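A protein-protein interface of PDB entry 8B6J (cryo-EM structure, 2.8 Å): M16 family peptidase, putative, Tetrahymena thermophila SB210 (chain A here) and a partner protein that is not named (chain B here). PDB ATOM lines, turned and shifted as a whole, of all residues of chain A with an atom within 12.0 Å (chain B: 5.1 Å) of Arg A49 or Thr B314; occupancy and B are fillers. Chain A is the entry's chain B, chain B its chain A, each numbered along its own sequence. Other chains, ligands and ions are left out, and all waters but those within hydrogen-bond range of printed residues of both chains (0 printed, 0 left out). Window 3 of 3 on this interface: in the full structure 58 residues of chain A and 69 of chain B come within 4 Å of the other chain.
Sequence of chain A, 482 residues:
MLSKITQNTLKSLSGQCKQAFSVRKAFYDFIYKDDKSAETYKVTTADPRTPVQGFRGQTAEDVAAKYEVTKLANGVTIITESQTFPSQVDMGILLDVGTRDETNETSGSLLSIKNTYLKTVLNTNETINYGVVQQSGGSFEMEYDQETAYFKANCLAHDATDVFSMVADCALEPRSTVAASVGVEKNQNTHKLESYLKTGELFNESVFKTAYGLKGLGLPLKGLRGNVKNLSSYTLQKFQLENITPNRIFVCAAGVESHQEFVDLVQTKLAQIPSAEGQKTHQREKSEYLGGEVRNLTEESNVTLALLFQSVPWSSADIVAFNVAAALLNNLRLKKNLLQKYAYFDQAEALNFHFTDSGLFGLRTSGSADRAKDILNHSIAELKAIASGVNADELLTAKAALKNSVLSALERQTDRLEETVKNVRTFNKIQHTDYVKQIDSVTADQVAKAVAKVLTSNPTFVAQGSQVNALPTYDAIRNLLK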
ATOM      1  N   LYS A  42     -16.196  23.084  14.380  1.00  0.00           N
ATOM      2  CA  LYS A  42     -16.063  24.160  13.404  1.00  0.00           C
ATOM      3  C   LYS A  42     -14.616  24.619  13.285  1.00  0.00           C
ATOM      4  O   LYS A  42     -14.119  24.851  12.178  1.00  0.00           O
ATOM      5  CB  LYS A  42     -16.963  25.333  13.790  1.00  0.00           C
ATOM      6  CG  LYS A  42     -18.443  25.020  13.721  1.00  0.00           C
ATOM      7  CD  LYS A  42     -19.282  26.243  14.033  1.00  0.00           C
ATOM      8  CE  LYS A  42     -20.766  25.942  13.924  1.00  0.00           C
ATOM      9  NZ  LYS A  42     -21.597  27.140  14.210  1.00  0.00           N
ATOM     10  N   VAL A  43     -13.923  24.760  14.417  1.00  0.00           N
ATOM     11  CA  VAL A  43     -12.538  25.222  14.381  1.00  0.00           C
ATOM     12  C   VAL A  43     -11.655  24.207  13.666  1.00  0.00           C
ATOM     13  O   VAL A  43     -10.814  24.571  12.836  1.00  0.00           O
ATOM     14  CB  VAL A  43     -12.032  25.507  15.805  1.00  0.00           C
ATOM     15  CG1 VAL A  43     -10.546  25.809  15.789  1.00  0.00           C
ATOM     16  CG2 VAL A  43     -12.798  26.666  16.418  1.00  0.00           C
ATOM     17  N   THR A  44     -11.827  22.922  13.977  1.00  0.00           N
ATOM     18  CA  THR A  44     -10.958  21.903  13.396  1.00  0.00           C
ATOM     19  C   THR A  44     -11.245  21.685  11.916  1.00  0.00           C
ATOM     20  O   THR A  44     -10.334  21.337  11.156  1.00  0.00           O
ATOM     21  CB  THR A  44     -11.104  20.588  14.159  1.00  0.00           C
ATOM     22  OG1 THR A  44     -12.479  20.188  14.168  1.00  0.00           O
ATOM     23  CG2 THR A  44     -10.613  20.747  15.588  1.00  0.00           C
ATOM     24  N   THR A  45     -12.492  21.875  11.485  1.00  0.00           N
ATOM     25  CA  THR A  45     -12.877  21.673  10.095  1.00  0.00           C
ATOM     26  C   THR A  45     -12.932  22.975   9.306  1.00  0.00           C
ATOM     27  O   THR A  45     -13.438  22.982   8.180  1.00  0.00           O
ATOM     28  CB  THR A  45     -14.231  20.966  10.015  1.00  0.00           C
ATOM     29  OG1 THR A  45     -15.225  21.744  10.691  1.00  0.00           O
ATOM     30  CG2 THR A  45     -14.150  19.585  10.643  1.00  0.00           C
ATOM     31  N   ALA A  46     -12.432  24.072   9.867  1.00  0.00           N
ATOM     32  CA  ALA A  46     -12.376  25.321   9.123  1.00  0.00           C
ATOM     33  C   ALA A  46     -11.459  25.170   7.915  1.00  0.00           C
ATOM     34  O   ALA A  46     -10.414  24.519   7.986  1.00  0.00           O
ATOM     35  CB  ALA A  46     -11.884  26.454  10.022  1.00  0.00           C
ATOM     36  N   ASP A  47     -11.855  25.775   6.804  1.00  0.00           N
ATOM     37  CA  ASP A  47     -11.090  25.643   5.574  1.00  0.00           C
ATOM     38  C   ASP A  47      -9.700  26.247   5.761  1.00  0.00           C
ATOM     39  O   ASP A  47      -9.582  27.360   6.292  1.00  0.00           O
ATOM     40  CB  ASP A  47     -11.815  26.333   4.422  1.00  0.00           C
ATOM     41  CG  ASP A  47     -11.159  26.073   3.081  1.00  0.00           C
ATOM     42  OD1 ASP A  47     -11.111  24.901   2.656  1.00  0.00           O
ATOM     43  OD2 ASP A  47     -10.694  27.043   2.451  1.00  0.00           O
ATOM     44  N   PRO A  48      -8.630  25.559   5.350  1.00  0.00           N
ATOM     45  CA  PRO A  48      -7.283  26.120   5.552  1.00  0.00           C
ATOM     46  C   PRO A  48      -7.043  27.421   4.812  1.00  0.00           C
ATOM     47  O   PRO A  48      -6.119  28.157   5.176  1.00  0.00           O
ATOM     48  CB  PRO A  48      -6.357  25.010   5.034  1.00  0.00           C
ATOM     49  CG  PRO A  48      -7.174  23.776   5.052  1.00  0.00           C
ATOM     50  CD  PRO A  48      -8.572  24.207   4.767  1.00  0.00           C
ATOM     51  N   ARG A  49      -7.836  27.729   3.784  1.00  0.00           N
ATOM     52  CA  ARG A  49      -7.573  28.918   2.981  1.00  0.00           C
ATOM     53  C   ARG A  49      -7.869  30.201   3.746  1.00  0.00           C
ATOM     54  O   ARG A  49      -7.287  31.247   3.435  1.00  0.00           O
ATOM     55  CB  ARG A  49      -8.403  28.880   1.699  1.00  0.00           C
ATOM     56  CG  ARG A  49      -8.223  27.620   0.874  1.00  0.00           C
ATOM     57  CD  ARG A  49      -9.224  27.576  -0.265  1.00  0.00           C
ATOM     58  NE  ARG A  49      -9.149  26.331  -1.017  1.00  0.00           N
ATOM     59  CZ  ARG A  49     -10.000  25.980  -1.970  1.00  0.00           C
ATOM     60  NH1 ARG A  49     -11.014  26.758  -2.310  1.00  0.00           N
ATOM     61  NH2 ARG A  49      -9.830  24.819  -2.597  1.00  0.00           N
ATOM     62  N   THR A  50      -8.755  30.149   4.734  1.00  0.00           N
ATOM     63  CA  THR A  50      -9.162  31.335   5.469  1.00  0.00           C
ATOM     64  C   THR A  50      -8.983  31.116   6.963  1.00  0.00           C
ATOM     65  O   THR A  50      -9.086  29.984   7.447  1.00  0.00           O
ATOM     66  CB  THR A  50     -10.627  31.691   5.183  1.00  0.00           C
ATOM     67  OG1 THR A  50     -11.461  30.557   5.452  1.00  0.00           O
ATOM     68  CG2 THR A  50     -10.803  32.116   3.733  1.00  0.00           C
ATOM     69  N   PRO A  51      -8.721  32.181   7.718  1.00  0.00           N
ATOM     70  CA  PRO A  51      -8.506  32.024   9.160  1.00  0.00           C
ATOM     71  C   PRO A  51      -9.773  31.599   9.881  1.00  0.00           C
ATOM     72  O   PRO A  51     -10.892  31.895   9.453  1.00  0.00           O
ATOM     73  CB  PRO A  51      -8.055  33.419   9.603  1.00  0.00           C
ATOM     74  CG  PRO A  51      -8.651  34.339   8.601  1.00  0.00           C
ATOM     75  CD  PRO A  51      -8.646  33.592   7.301  1.00  0.00           C
ATOM     76  N   VAL A  52      -9.584  30.891  10.997  1.00  0.00           N
ATOM     77  CA  VAL A  52     -10.721  30.481  11.809  1.00  0.00           C
ATOM     78  C   VAL A  52     -11.427  31.718  12.341  1.00  0.00           C
ATOM     79  O   VAL A  52     -10.791  32.675  12.801  1.00  0.00           O
ATOM     80  CB  VAL A  52     -10.268  29.561  12.954  1.00  0.00           C
ATOM     81  CG1 VAL A  52      -9.521  28.357  12.406  1.00  0.00           C
ATOM     82  CG2 VAL A  52      -9.409  30.323  13.943  1.00  0.00           C
ATOM     83  N   GLN A  53     -12.755  31.703  12.278  1.00  0.00           N
ATOM     84  CA  GLN A  53     -13.534  32.868  12.672  1.00  0.00           C
ATOM     85  C   GLN A  53     -13.400  33.116  14.169  1.00  0.00           C
ATOM     86  O   GLN A  53     -13.557  32.200  14.981  1.00  0.00           O
ATOM     87  CB  GLN A  53     -15.002  32.669  12.297  1.00  0.00           C
ATOM     88  CG  GLN A  53     -15.889  33.871  12.584  1.00  0.00           C
ATOM     89  CD  GLN A  53     -15.425  35.125  11.866  1.00  0.00           C
ATOM     90  OE1 GLN A  53     -14.519  35.818  12.327  1.00  0.00           O
ATOM     91  NE2 GLN A  53     -16.045  35.417  10.729  1.00  0.00           N
ATOM     92  N   PHE A  55     -10.690  34.212  15.910  1.00  0.00           N
ATOM     93  CA  PHE A  55      -9.336  34.163  16.445  1.00  0.00           C
ATOM     94  C   PHE A  55      -8.409  34.992  15.571  1.00  0.00           C
ATOM     95  O   PHE A  55      -8.415  34.853  14.344  1.00  0.00           O
ATOM     96  CB  PHE A  55      -8.830  32.722  16.528  1.00  0.00           C
ATOM     97  CG  PHE A  55      -7.482  32.595  17.172  1.00  0.00           C
ATOM     98  CD1 PHE A  55      -7.361  32.538  18.549  1.00  0.00           C
ATOM     99  CD2 PHE A  55      -6.336  32.531  16.403  1.00  0.00           C
ATOM    100  CE1 PHE A  55      -6.122  32.421  19.144  1.00  0.00           C
ATOM    101  CE2 PHE A  55      -5.095  32.414  16.994  1.00  0.00           C
ATOM    102  CZ  PHE A  55      -4.989  32.359  18.365  1.00  0.00           C
ATOM    103  N   SER B 312      -5.638  16.755   0.943  1.00  0.00           N
ATOM    104  CA  SER B 312      -4.842  17.694   0.174  1.00  0.00           C
ATOM    105  C   SER B 312      -4.561  18.937   1.013  1.00  0.00           C
ATOM    106  O   SER B 312      -4.995  19.059   2.160  1.00  0.00           O
ATOM    107  CB  SER B 312      -5.559  18.052  -1.129  1.00  0.00           C
ATOM    108  OG  SER B 312      -6.858  18.553  -0.876  1.00  0.00           O
ATOM    109  N   TRP B 313      -3.819  19.877   0.425  1.00  0.00           N
ATOM    110  CA  TRP B 313      -3.482  21.104   1.139  1.00  0.00           C
ATOM    111  C   TRP B 313      -4.724  21.896   1.522  1.00  0.00           C
ATOM    112  O   TRP B 313      -4.733  22.572   2.557  1.00  0.00           O
ATOM    113  CB  TRP B 313      -2.553  21.969   0.287  1.00  0.00           C
ATOM    114  CG  TRP B 313      -1.103  21.723   0.536  1.00  0.00           C
ATOM    115  CD1 TRP B 313      -0.315  20.786  -0.060  1.00  0.00           C
ATOM    116  CD2 TRP B 313      -0.259  22.434   1.447  1.00  0.00           C
ATOM    117  NE1 TRP B 313       0.966  20.866   0.425  1.00  0.00           N
ATOM    118  CE2 TRP B 313       1.026  21.871   1.353  1.00  0.00           C
ATOM    119  CE3 TRP B 313      -0.467  23.492   2.336  1.00  0.00           C
ATOM    120  CZ2 TRP B 313       2.097  22.330   2.110  1.00  0.00           C
ATOM    121  CZ3 TRP B 313       0.596  23.946   3.087  1.00  0.00           C
ATOM    122  CH2 TRP B 313       1.862  23.366   2.970  1.00  0.00           C
ATOM    123  N   THR B 314      -5.773  21.837   0.705  1.00  0.00           N
ATOM    124  CA  THR B 314      -6.972  22.635   0.913  1.00  0.00           C
ATOM    125  C   THR B 314      -8.102  21.849   1.562  1.00  0.00           C
ATOM    126  O   THR B 314      -9.218  22.367   1.673  1.00  0.00           O
ATOM    127  CB  THR B 314      -7.449  23.216  -0.418  1.00  0.00           C
ATOM    128  OG1 THR B 314      -7.735  22.151  -1.333  1.00  0.00           O
ATOM    129  CG2 THR B 314      -6.386  24.125  -1.016  1.00  0.00           C
ATOM    130  N   ASP B 315      -7.849  20.616   1.985  1.00  0.00           N
ATOM    131  CA  ASP B 315      -8.891  19.827   2.617  1.00  0.00           C
ATOM    132  C   ASP B 315      -9.136  20.315   4.045  1.00  0.00           C
ATOM    133  O   ASP B 315      -8.213  20.791   4.710  1.00  0.00           O
ATOM    134  CB  ASP B 315      -8.503  18.355   2.636  1.00  0.00           C
ATOM    135  CG  ASP B 315      -9.703  17.439   2.702  1.00  0.00           C
ATOM    136  OD1 ASP B 315     -10.383  17.276   1.668  1.00  0.00           O
ATOM    137  OD2 ASP B 315      -9.971  16.881   3.786  1.00  0.00           O
ATOM    138  N   PRO B 316     -10.374  20.214   4.542  1.00  0.00           N
ATOM    139  CA  PRO B 316     -10.622  20.637   5.930  1.00  0.00           C
ATOM    140  C   PRO B 316      -9.767  19.900   6.946  1.00  0.00           C
ATOM    141  O   PRO B 316      -9.336  20.502   7.938  1.00  0.00           O
ATOM    142  CB  PRO B 316     -12.116  20.341   6.121  1.00  0.00           C
ATOM    143  CG  PRO B 316     -12.685  20.367   4.755  1.00  0.00           C
ATOM    144  CD  PRO B 316     -11.619  19.820   3.861  1.00  0.00           C
ATOM    145  N   SER B 372      -1.825  19.146  -4.185  1.00  0.00           N
ATOM    146  CA  SER B 372      -2.948  19.986  -4.583  1.00  0.00           C
ATOM    147  C   SER B 372      -4.256  19.206  -4.580  1.00  0.00           C
ATOM    148  O   SER B 372      -5.291  19.719  -4.139  1.00  0.00           O
ATOM    149  CB  SER B 372      -2.687  20.584  -5.964  1.00  0.00           C
ATOM    150  OG  SER B 372      -2.527  19.566  -6.935  1.00  0.00           O
ATOM    151  N   TYR B 441       0.355  26.853  -2.021  1.00  0.00           N
ATOM    152  CA  TYR B 441      -0.738  25.893  -1.931  1.00  0.00           C
ATOM    153  C   TYR B 441      -1.981  26.435  -1.237  1.00  0.00           C
ATOM    154  O   TYR B 441      -3.016  25.763  -1.255  1.00  0.00           O
ATOM    155  CB  TYR B 441      -0.273  24.630  -1.204  1.00  0.00           C
ATOM    156  CG  TYR B 441       0.538  23.695  -2.067  1.00  0.00           C
ATOM    157  CD1 TYR B 441      -0.058  22.979  -3.095  1.00  0.00           C
ATOM    158  CD2 TYR B 441       1.895  23.517  -1.849  1.00  0.00           C
ATOM    159  CE1 TYR B 441       0.675  22.121  -3.885  1.00  0.00           C
ATOM    160  CE2 TYR B 441       2.637  22.659  -2.633  1.00  0.00           C
ATOM    161  CZ  TYR B 441       2.021  21.963  -3.649  1.00  0.00           C
ATOM    162  OH  TYR B 441       2.758  21.108  -4.433  1.00  0.00           O
ATOM    163  N   LEU B 442      -1.914  27.621  -0.634  1.00  0.00           N
ATOM    164  CA  LEU B 442      -3.057  28.202   0.054  1.00  0.00           C
ATOM    165  C   LEU B 442      -3.279  29.672  -0.259  1.00  0.00           C
ATOM    166  O   LEU B 442      -4.312  30.216   0.145  1.00  0.00           O
ATOM    167  CB  LEU B 442      -2.903  28.049   1.576  1.00  0.00           C
ATOM    168  CG  LEU B 442      -2.824  26.622   2.118  1.00  0.00           C
ATOM    169  CD1 LEU B 442      -2.468  26.640   3.592  1.00  0.00           C
ATOM    170  CD2 LEU B 442      -4.133  25.890   1.898  1.00  0.00           C
ATOM    171  N   ARG B 444      -1.836  32.086   1.085  1.00  0.00           N
ATOM    172  CA  ARG B 444      -1.903  32.697   2.403  1.00  0.00           C
ATOM    173  C   ARG B 444      -0.787  32.135   3.267  1.00  0.00           C
ATOM    174  O   ARG B 444      -0.405  30.971   3.128  1.00  0.00           O
ATOM    175  CB  ARG B 444      -3.263  32.439   3.063  1.00  0.00           C
ATOM    176  CG  ARG B 444      -3.431  33.088   4.422  1.00  0.00           C
ATOM    177  CD  ARG B 444      -4.828  32.853   4.968  1.00  0.00           C
ATOM    178  NE  ARG B 444      -5.035  31.468   5.376  1.00  0.00           N
ATOM    179  CZ  ARG B 444      -4.848  31.009   6.606  1.00  0.00           C
ATOM    180  NH1 ARG B 444      -4.440  31.797   7.587  1.00  0.00           N
ATOM    181  NH2 ARG B 444      -5.077  29.724   6.859  1.00  0.00           N
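Of the printed residues of chain B, Thr A44 touches Pro B316.
Ala A46 touches none of the printed residues of chain B.
Of the printed residues of chain B, Pro A48 touches Trp B313, Thr B314, Asp B315, Leu B442 and Arg B444.
Of chain B, only Thr B314 and Arg B444 come within 4 Å of Arg A49.
Printed residues of chain B within 4 Å of Thr A50: Arg B444 (3.999 Å).
Pro A51 touches none of the printed residues of chain B.
No residue of chain A comes within 4 Å of Ser B312.
Of chain A, only Asp A47 (3.3 Å), Pro A48 (3.7 Å) and Arg A49 (3.5 Å) come within 4 Å of Thr B314.
Asp B315 touches just one residue of chain A: Pro A48 (3.2 Å).
Pro B316 touches just these residues of chain A: Thr A44 and Thr A45.
Of chain A, only Pro A48 comes within 4 Å of Leu B442.
Of the printed residues of chain A, Arg B444 touches Pro A48, Arg A49 and Thr A50.
The nearest residue of chain B that does not touch Arg A49 is Leu B442 (4.5 Å).
The nearest residue of chain A that does not touch Thr B314 is Ala A46 (6.8 Å).
The nearest printed residue of chain B that does not touch Asp A47 is Pro B316 (5.0 Å).
Hydrophobic or aromatic side chains of chain A within 4 Å of the printed part of chain B: Pro A48.
Of the 9 printed residues of chain B, 6 touch a printed residue of chain A.
Among the printed residues, 11 pairs touch across the chains.
OD2 of Asp A47 is in salt-bridge range of NE of Arg A49 (3.9 Å).
O of Thr A45 touches CB of Pro B316, at 3.6 Å.
Trp B313 touches Pro A48.
Pro A48 touches Thr B314 (CD to O, 3.7 Å).
Asp B315 touches Pro A48 (O to CG, 3.2 Å).
Pro A48 touches Leu B442 (CB to CD2, 3.9 Å).
CG2 of Thr B314 touches NE of Arg A49 (3.5 Å).
Arg B444 touches Thr A50.
OD1 of Asp A47 lies close to O of Thr B314, at 3.3 Å.
The backbone carbonyl oxygen of Thr A44 sits close to the backbone carbonyl oxygen of Pro B316 (3.5 Å).
The backbone carbonyl oxygen (O) of Pro A48 lies within hydrogen-bond range of the guanidinium group (NH2) of Arg B444, 2.5 Å away.
The backbone carbonyl oxygen (O) of Arg A49 sits at hydrogen-bond distance from the guanidinium group (NE) of Arg B444, 3.0 Å away.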
